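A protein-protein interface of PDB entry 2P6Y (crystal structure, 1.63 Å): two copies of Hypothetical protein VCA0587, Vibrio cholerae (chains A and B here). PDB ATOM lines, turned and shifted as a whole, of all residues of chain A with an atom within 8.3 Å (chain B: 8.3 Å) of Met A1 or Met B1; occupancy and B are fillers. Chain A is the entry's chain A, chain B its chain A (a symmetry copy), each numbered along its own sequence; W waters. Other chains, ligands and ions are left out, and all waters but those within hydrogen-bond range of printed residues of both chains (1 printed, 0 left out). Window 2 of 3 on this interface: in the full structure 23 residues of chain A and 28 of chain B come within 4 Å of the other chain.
Water W1 bridges the backbone NH of Ile B2 (2.9 Å) and the backbone carbonyl oxygen of Ile A2 (3.0 Å).
Ile A2 touches its own counterpart, Ile B2.
Leu A4 touches Tyr B109, but with the chains exchanged Tyr A109 does not touch Leu B4 (12.9 Å).
Leu A4 touches His B112, but with the chains exchanged His A112 does not touch Leu B4 (16.7 Å).
His A107 touches Ile B2, but with the chains exchanged Ile A2 does not touch His B107 (6.7 Å).
10 positions are printed for both chains.
Of the 7 pairs that touch across the chains among the printed residues, 3 have their exchanged pair printed and touching as well.
Among the printed residues, pairs that only touch across the chains: Met A1 with Met B1 (2.9 Å), Ile A2 with Ile B2 (3.7 Å), Leu A4 with Tyr B109 (3.4 Å), Leu A4 with His B112 (3.6 Å), His A107 with Ile B2 (3.9 Å) and His A107 with His B107 (3.8 Å).
Of the 10 printed residues of chain B, 5 touch a printed residue of chain A.
Hydrophobic or aromatic side chains of chain B within 4 Å of the printed part of chain A: Met B1, Ile B2, His B107, Tyr B109 and His B112.
Hydrophobic or aromatic side chains of chain A within 4 Å of the printed part of chain B: Met A1, Ile A2, Leu A4 and His A107.
Among the printed residues, no Asp or Glu carboxylate lies within 4 Å of a Lys or Arg side-chain nitrogen of the other chain.
A ring nitrogen (NE2) of His A107 sits at hydrogen-bond distance from the side-chain hydroxyl (OH) of Tyr B109.
Met A1 touches one residue of chain B.
Met B1 touches just one residue of chain A: Met A1.
Printed residues of chain B within 4 Å of His A107: Ile B2 (3.9 Å), His B107 (3.8 Å) and Tyr B109 (3.0 Å).
Of the printed residues of chain A, His B107 touches His A107 (3.8 Å).
Printed residues of chain B within 4 Å of Leu A4: Tyr B109 and His B112.
Of the printed residues of chain A, Tyr B109 touches Leu A4 and His A107.
Of the printed residues of chain A, Ile B2 touches Ile A2 and His A107.
His B3 touches none of the printed residues of chain A.
The nearest residue of chain B that does not touch Met A1 is Ile B2 (5.6 Å).
The nearest residue of chain A that does not touch Met B1 is Ile A2 (5.5 Å).
The nearest printed residue of chain B that does not touch His A107 is His B108 (8.0 Å).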
ATOM      1  N   MET A   1      -7.555 -18.086  17.664  1.00  0.00           N
ATOM      2  CA  MET A   1      -7.291 -19.089  16.596  1.00  0.00           C
ATOM      3  C   MET A   1      -8.406 -20.128  16.555  1.00  0.00           C
ATOM      4  O   MET A   1      -8.847 -20.616  17.596  1.00  0.00           O
ATOM      5  CB  MET A   1      -5.954 -19.789  16.850  1.00  0.00           C
ATOM      6  CG  MET A   1      -5.571 -20.802  15.785  1.00  0.00           C
ATOM      7  SD  MET A   1      -3.956 -21.771  16.215  1.00  0.00           S
ATOM      8  CE  MET A   1      -2.661 -20.509  15.530  1.00  0.00           C
ATOM      9  N   ILE A   2      -8.855 -20.463  15.350  1.00  0.00           N
ATOM     10  CA  ILE A   2      -9.915 -21.449  15.178  1.00  0.00           C
ATOM     11  C   ILE A   2      -9.372 -22.845  15.465  1.00  0.00           C
ATOM     12  O   ILE A   2      -8.315 -23.225  14.960  1.00  0.00           O
ATOM     13  CB  ILE A   2     -10.474 -21.429  13.740  1.00  0.00           C
ATOM     14  CG1 ILE A   2     -10.940 -20.015  13.381  1.00  0.00           C
ATOM     15  CG2 ILE A   2     -11.630 -22.408  13.619  1.00  0.00           C
ATOM     16  CD1 ILE A   2     -11.410 -19.875  11.947  1.00  0.00           C
ATOM     17  N   HIS A   3     -10.100 -23.604  16.277  1.00  0.00           N
ATOM     18  CA  HIS A   3      -9.692 -24.956  16.630  1.00  0.00           C
ATOM     19  C   HIS A   3     -10.629 -25.999  16.035  1.00  0.00           C
ATOM     20  O   HIS A   3     -11.833 -25.773  15.916  1.00  0.00           O
ATOM     21  CB  HIS A   3      -9.648 -25.113  18.152  1.00  0.00           C
ATOM     22  CG  HIS A   3      -8.588 -24.285  18.812  1.00  0.00           C
ATOM     23  ND1 HIS A   3      -8.460 -24.194  20.181  1.00  0.00           N
ATOM     24  CD2 HIS A   3      -7.605 -23.515  18.290  1.00  0.00           C
ATOM     25  CE1 HIS A   3      -7.444 -23.401  20.474  1.00  0.00           C
ATOM     26  NE2 HIS A   3      -6.908 -22.976  19.345  1.00  0.00           N
ATOM     27  N   LEU A   4     -10.062 -27.142  15.661  1.00  0.00           N
ATOM     28  CA  LEU A   4     -10.833 -28.235  15.086  1.00  0.00           C
ATOM     29  C   LEU A   4     -11.059 -29.357  16.082  1.00  0.00           C
ATOM     30  O   LEU A   4     -10.147 -29.758  16.805  1.00  0.00           O
ATOM     31  CB  LEU A   4     -10.121 -28.833  13.869  1.00  0.00           C
ATOM     32  CG  LEU A   4     -10.693 -30.196  13.440  1.00  0.00           C
ATOM     33  CD1 LEU A   4     -12.001 -29.987  12.693  1.00  0.00           C
ATOM     34  CD2 LEU A   4      -9.699 -30.938  12.560  1.00  0.00           C
ATOM     35  N   HIS A 107     -15.786 -26.512  14.328  1.00  0.00           N
ATOM     36  CA  HIS A 107     -14.803 -25.448  14.451  1.00  0.00           C
ATOM     37  C   HIS A 107     -15.168 -24.671  15.709  1.00  0.00           C
ATOM     38  O   HIS A 107     -16.313 -24.246  15.878  1.00  0.00           O
ATOM     39  CB  HIS A 107     -14.823 -24.548  13.209  1.00  0.00           C
ATOM     40  CG  HIS A 107     -14.091 -25.126  12.035  1.00  0.00           C
ATOM     41  ND1 HIS A 107     -14.143 -24.570  10.775  1.00  0.00           N
ATOM     42  CD2 HIS A 107     -13.272 -26.201  11.936  1.00  0.00           C
ATOM     43  CE1 HIS A 107     -13.388 -25.274   9.952  1.00  0.00           C
ATOM     44  NE2 HIS A 107     -12.847 -26.269  10.630  1.00  0.00           N
ATOM     45  N   HIS A 108     -14.193 -24.527  16.604  1.00  0.00           N
ATOM     46  CA  HIS A 108     -14.368 -23.826  17.873  1.00  0.00           C
ATOM     47  C   HIS A 108     -13.650 -22.483  17.796  1.00  0.00           C
ATOM     48  O   HIS A 108     -12.506 -22.409  17.353  1.00  0.00           O
ATOM     49  CB  HIS A 108     -13.809 -24.710  19.006  1.00  0.00           C
ATOM     50  CG  HIS A 108     -13.673 -24.020  20.329  1.00  0.00           C
ATOM     51  ND1 HIS A 108     -14.571 -23.078  20.783  1.00  0.00           N
ATOM     52  CD2 HIS A 108     -12.767 -24.182  21.322  1.00  0.00           C
ATOM     53  CE1 HIS A 108     -14.223 -22.688  21.998  1.00  0.00           C
ATOM     54  NE2 HIS A 108     -13.132 -23.343  22.347  1.00  0.00           N
ATOM     55  N   TYR A 109     -14.338 -21.422  18.206  1.00  0.00           N
ATOM     56  CA  TYR A 109     -13.780 -20.072  18.175  1.00  0.00           C
ATOM     57  C   TYR A 109     -13.585 -19.573  19.605  1.00  0.00           C
ATOM     58  O   TYR A 109     -14.459 -18.906  20.160  1.00  0.00           O
ATOM     59  CB  TYR A 109     -14.738 -19.135  17.438  1.00  0.00           C
ATOM     60  CG  TYR A 109     -15.183 -19.644  16.085  1.00  0.00           C
ATOM     61  CD1 TYR A 109     -14.277 -19.797  15.042  1.00  0.00           C
ATOM     62  CD2 TYR A 109     -16.515 -19.963  15.846  1.00  0.00           C
ATOM     63  CE1 TYR A 109     -14.686 -20.258  13.788  1.00  0.00           C
ATOM     64  CE2 TYR A 109     -16.937 -20.425  14.596  1.00  0.00           C
ATOM     65  CZ  TYR A 109     -16.018 -20.569  13.574  1.00  0.00           C
ATOM     66  OH  TYR A 109     -16.425 -21.022  12.334  1.00  0.00           O
ATOM     67  N   PRO A 110     -12.428 -19.879  20.213  1.00  0.00           N
ATOM     68  CA  PRO A 110     -12.092 -19.480  21.586  1.00  0.00           C
ATOM     69  C   PRO A 110     -12.124 -17.979  21.862  1.00  0.00           C
ATOM     70  O   PRO A 110     -12.334 -17.558  23.000  1.00  0.00           O
ATOM     71  CB  PRO A 110     -10.688 -20.053  21.779  1.00  0.00           C
ATOM     72  CG  PRO A 110     -10.677 -21.245  20.879  1.00  0.00           C
ATOM     73  CD  PRO A 110     -11.353 -20.707  19.640  1.00  0.00           C
ATOM     74  N   GLN A 111     -11.919 -17.182  20.821  1.00  0.00           N
ATOM     75  CA  GLN A 111     -11.889 -15.731  20.948  1.00  0.00           C
ATOM     76  C   GLN A 111     -13.277 -15.091  20.877  1.00  0.00           C
ATOM     77  O   GLN A 111     -13.420 -13.876  21.036  1.00  0.00           O
ATOM     78  CB  GLN A 111     -10.986 -15.153  19.853  1.00  0.00           C
ATOM     79  CG  GLN A 111     -10.539 -13.722  20.070  1.00  0.00           C
ATOM     80  CD  GLN A 111      -9.621 -13.236  18.963  1.00  0.00           C
ATOM     81  OE1 GLN A 111      -8.598 -13.860  18.669  1.00  0.00           O
ATOM     82  NE2 GLN A 111      -9.982 -12.117  18.343  1.00  0.00           N
ATOM     83  N   HIS A 112     -14.297 -15.909  20.640  1.00  0.00           N
ATOM     84  CA  HIS A 112     -15.665 -15.412  20.548  1.00  0.00           C
ATOM     85  C   HIS A 112     -16.575 -15.988  21.621  1.00  0.00           C
ATOM     86  O   HIS A 112     -16.268 -17.003  22.245  1.00  0.00           O
ATOM     87  CB  HIS A 112     -16.270 -15.738  19.178  1.00  0.00           C
ATOM     88  CG  HIS A 112     -15.673 -14.957  18.050  1.00  0.00           C
ATOM     89  ND1 HIS A 112     -14.404 -15.195  17.567  1.00  0.00           N
ATOM     90  CD2 HIS A 112     -16.167 -13.929  17.320  1.00  0.00           C
ATOM     91  CE1 HIS A 112     -14.142 -14.347  16.588  1.00  0.00           C
ATOM     92  NE2 HIS A 112     -15.196 -13.568  16.419  1.00  0.00           N
ATOM     93  N   MET B   1      -2.542 -24.974  13.460  1.00  0.00           N
ATOM     94  CA  MET B   1      -3.301 -23.885  12.785  1.00  0.00           C
ATOM     95  C   MET B   1      -3.903 -24.388  11.478  1.00  0.00           C
ATOM     96  O   MET B   1      -3.239 -25.082  10.707  1.00  0.00           O
ATOM     97  CB  MET B   1      -2.375 -22.701  12.495  1.00  0.00           C
ATOM     98  CG  MET B   1      -3.068 -21.515  11.847  1.00  0.00           C
ATOM     99  SD  MET B   1      -1.844 -20.102  11.359  1.00  0.00           S
ATOM    100  CE  MET B   1      -1.769 -19.176  13.055  1.00  0.00           C
ATOM    101  N   ILE B   2      -5.161 -24.032  11.234  1.00  0.00           N
ATOM    102  CA  ILE B   2      -5.846 -24.445  10.016  1.00  0.00           C
ATOM    103  C   ILE B   2      -5.299 -23.666   8.826  1.00  0.00           C
ATOM    104  O   ILE B   2      -5.171 -22.442   8.880  1.00  0.00           O
ATOM    105  CB  ILE B   2      -7.366 -24.187  10.112  1.00  0.00           C
ATOM    106  CG1 ILE B   2      -7.935 -24.876  11.355  1.00  0.00           C
ATOM    107  CG2 ILE B   2      -8.059 -24.704   8.862  1.00  0.00           C
ATOM    108  CD1 ILE B   2      -9.405 -24.591  11.589  1.00  0.00           C
ATOM    109  N   HIS B   3      -4.977 -24.379   7.753  1.00  0.00           N
ATOM    110  CA  HIS B   3      -4.444 -23.755   6.551  1.00  0.00           C
ATOM    111  C   HIS B   3      -5.425 -23.841   5.390  1.00  0.00           C
ATOM    112  O   HIS B   3      -6.159 -24.819   5.254  1.00  0.00           O
ATOM    113  CB  HIS B   3      -3.121 -24.416   6.156  1.00  0.00           C
ATOM    114  CG  HIS B   3      -2.015 -24.189   7.142  1.00  0.00           C
ATOM    115  ND1 HIS B   3      -0.783 -24.795   7.031  1.00  0.00           N
ATOM    116  CD2 HIS B   3      -1.958 -23.419   8.253  1.00  0.00           C
ATOM    117  CE1 HIS B   3      -0.013 -24.409   8.033  1.00  0.00           C
ATOM    118  NE2 HIS B   3      -0.702 -23.574   8.790  1.00  0.00           N
ATOM    119  N   LEU B   4      -5.431 -22.805   4.557  1.00  0.00           N
ATOM    120  CA  LEU B   4      -6.309 -22.751   3.397  1.00  0.00           C
ATOM    121  C   LEU B   4      -5.563 -23.028   2.106  1.00  0.00           C
ATOM    122  O   LEU B   4      -4.464 -22.520   1.885  1.00  0.00           O
ATOM    123  CB  LEU B   4      -6.966 -21.373   3.264  1.00  0.00           C
ATOM    124  CG  LEU B   4      -7.611 -21.139   1.887  1.00  0.00           C
ATOM    125  CD1 LEU B   4      -8.935 -21.885   1.811  1.00  0.00           C
ATOM    126  CD2 LEU B   4      -7.832 -19.653   1.647  1.00  0.00           C
ATOM    127  N   HIS B 107      -9.568 -26.922   3.625  1.00  0.00           N
ATOM    128  CA  HIS B 107      -8.965 -26.573   4.901  1.00  0.00           C
ATOM    129  C   HIS B 107      -8.094 -27.758   5.301  1.00  0.00           C
ATOM    130  O   HIS B 107      -8.555 -28.901   5.320  1.00  0.00           O
ATOM    131  CB  HIS B 107     -10.047 -26.292   5.952  1.00  0.00           C
ATOM    132  CG  HIS B 107     -10.657 -24.927   5.836  1.00  0.00           C
ATOM    133  ND1 HIS B 107     -11.766 -24.541   6.558  1.00  0.00           N
ATOM    134  CD2 HIS B 107     -10.297 -23.849   5.097  1.00  0.00           C
ATOM    135  CE1 HIS B 107     -12.063 -23.287   6.271  1.00  0.00           C
ATOM    136  NE2 HIS B 107     -11.188 -22.843   5.388  1.00  0.00           N
ATOM    137  N   HIS B 108      -6.824 -27.474   5.580  1.00  0.00           N
ATOM    138  CA  HIS B 108      -5.844 -28.486   5.964  1.00  0.00           C
ATOM    139  C   HIS B 108      -5.553 -28.347   7.455  1.00  0.00           C
ATOM    140  O   HIS B 108      -5.334 -27.243   7.951  1.00  0.00           O
ATOM    141  CB  HIS B 108      -4.573 -28.291   5.113  1.00  0.00           C
ATOM    142  CG  HIS B 108      -3.384 -29.077   5.573  1.00  0.00           C
ATOM    143  ND1 HIS B 108      -3.479 -30.347   6.102  1.00  0.00           N
ATOM    144  CD2 HIS B 108      -2.062 -28.790   5.527  1.00  0.00           C
ATOM    145  CE1 HIS B 108      -2.268 -30.806   6.365  1.00  0.00           C
ATOM    146  NE2 HIS B 108      -1.390 -29.880   6.025  1.00  0.00           N
ATOM    147  N   TYR B 109      -5.577 -29.469   8.168  1.00  0.00           N
ATOM    148  CA  TYR B 109      -5.332 -29.483   9.608  1.00  0.00           C
ATOM    149  C   TYR B 109      -4.018 -30.209   9.889  1.00  0.00           C
ATOM    150  O   TYR B 109      -4.011 -31.413  10.150  1.00  0.00           O
ATOM    151  CB  TYR B 109      -6.474 -30.211  10.319  1.00  0.00           C
ATOM    152  CG  TYR B 109      -7.853 -29.718   9.940  1.00  0.00           C
ATOM    153  CD1 TYR B 109      -8.266 -28.428  10.252  1.00  0.00           C
ATOM    154  CD2 TYR B 109      -8.749 -30.548   9.274  1.00  0.00           C
ATOM    155  CE1 TYR B 109      -9.542 -27.973   9.911  1.00  0.00           C
ATOM    156  CE2 TYR B 109     -10.028 -30.104   8.927  1.00  0.00           C
ATOM    157  CZ  TYR B 109     -10.417 -28.818   9.249  1.00  0.00           C
ATOM    158  OH  TYR B 109     -11.680 -28.371   8.914  1.00  0.00           O
ATOM    159  N   PRO B 110      -2.891 -29.481   9.851  1.00  0.00           N
ATOM    160  CA  PRO B 110      -1.551 -30.031  10.092  1.00  0.00           C
ATOM    161  C   PRO B 110      -1.353 -30.720  11.440  1.00  0.00           C
ATOM    162  O   PRO B 110      -0.499 -31.597  11.575  1.00  0.00           O
ATOM    163  CB  PRO B 110      -0.644 -28.809   9.952  1.00  0.00           C
ATOM    164  CG  PRO B 110      -1.389 -27.938   8.993  1.00  0.00           C
ATOM    165  CD  PRO B 110      -2.805 -28.052   9.504  1.00  0.00           C
ATOM    166  N   GLN B 111      -2.145 -30.322  12.428  1.00  0.00           N
ATOM    167  CA  GLN B 111      -2.042 -30.870  13.775  1.00  0.00           C
ATOM    168  C   GLN B 111      -2.836 -32.164  13.962  1.00  0.00           C
ATOM    169  O   GLN B 111      -2.793 -32.782  15.028  1.00  0.00           O
ATOM    170  CB  GLN B 111      -2.511 -29.813  14.780  1.00  0.00           C
ATOM    171  CG  GLN B 111      -2.112 -30.066  16.219  1.00  0.00           C
ATOM    172  CD  GLN B 111      -2.583 -28.959  17.146  1.00  0.00           C
ATOM    173  OE1 GLN B 111      -2.290 -27.782  16.925  1.00  0.00           O
ATOM    174  NE2 GLN B 111      -3.316 -29.333  18.190  1.00  0.00           N
ATOM    175  N   HIS B 112      -3.560 -32.572  12.924  1.00  0.00           N
ATOM    176  CA  HIS B 112      -4.360 -33.789  12.987  1.00  0.00           C
ATOM    177  C   HIS B 112      -3.913 -34.841  11.984  1.00  0.00           C
ATOM    178  O   HIS B 112      -3.206 -34.549  11.021  1.00  0.00           O
ATOM    179  CB  HIS B 112      -5.840 -33.479  12.732  1.00  0.00           C
ATOM    180  CG  HIS B 112      -6.500 -32.722  13.840  1.00  0.00           C
ATOM    181  ND1 HIS B 112      -6.246 -31.390  14.089  1.00  0.00           N
ATOM    182  CD2 HIS B 112      -7.395 -33.115  14.777  1.00  0.00           C
ATOM    183  CE1 HIS B 112      -6.955 -30.995  15.131  1.00  0.00           C
ATOM    184  NE2 HIS B 112      -7.660 -32.023  15.567  1.00  0.00           N
HETATM  185  O   HOH W   1      -6.318 -22.086  13.087  1.00  0.00           O
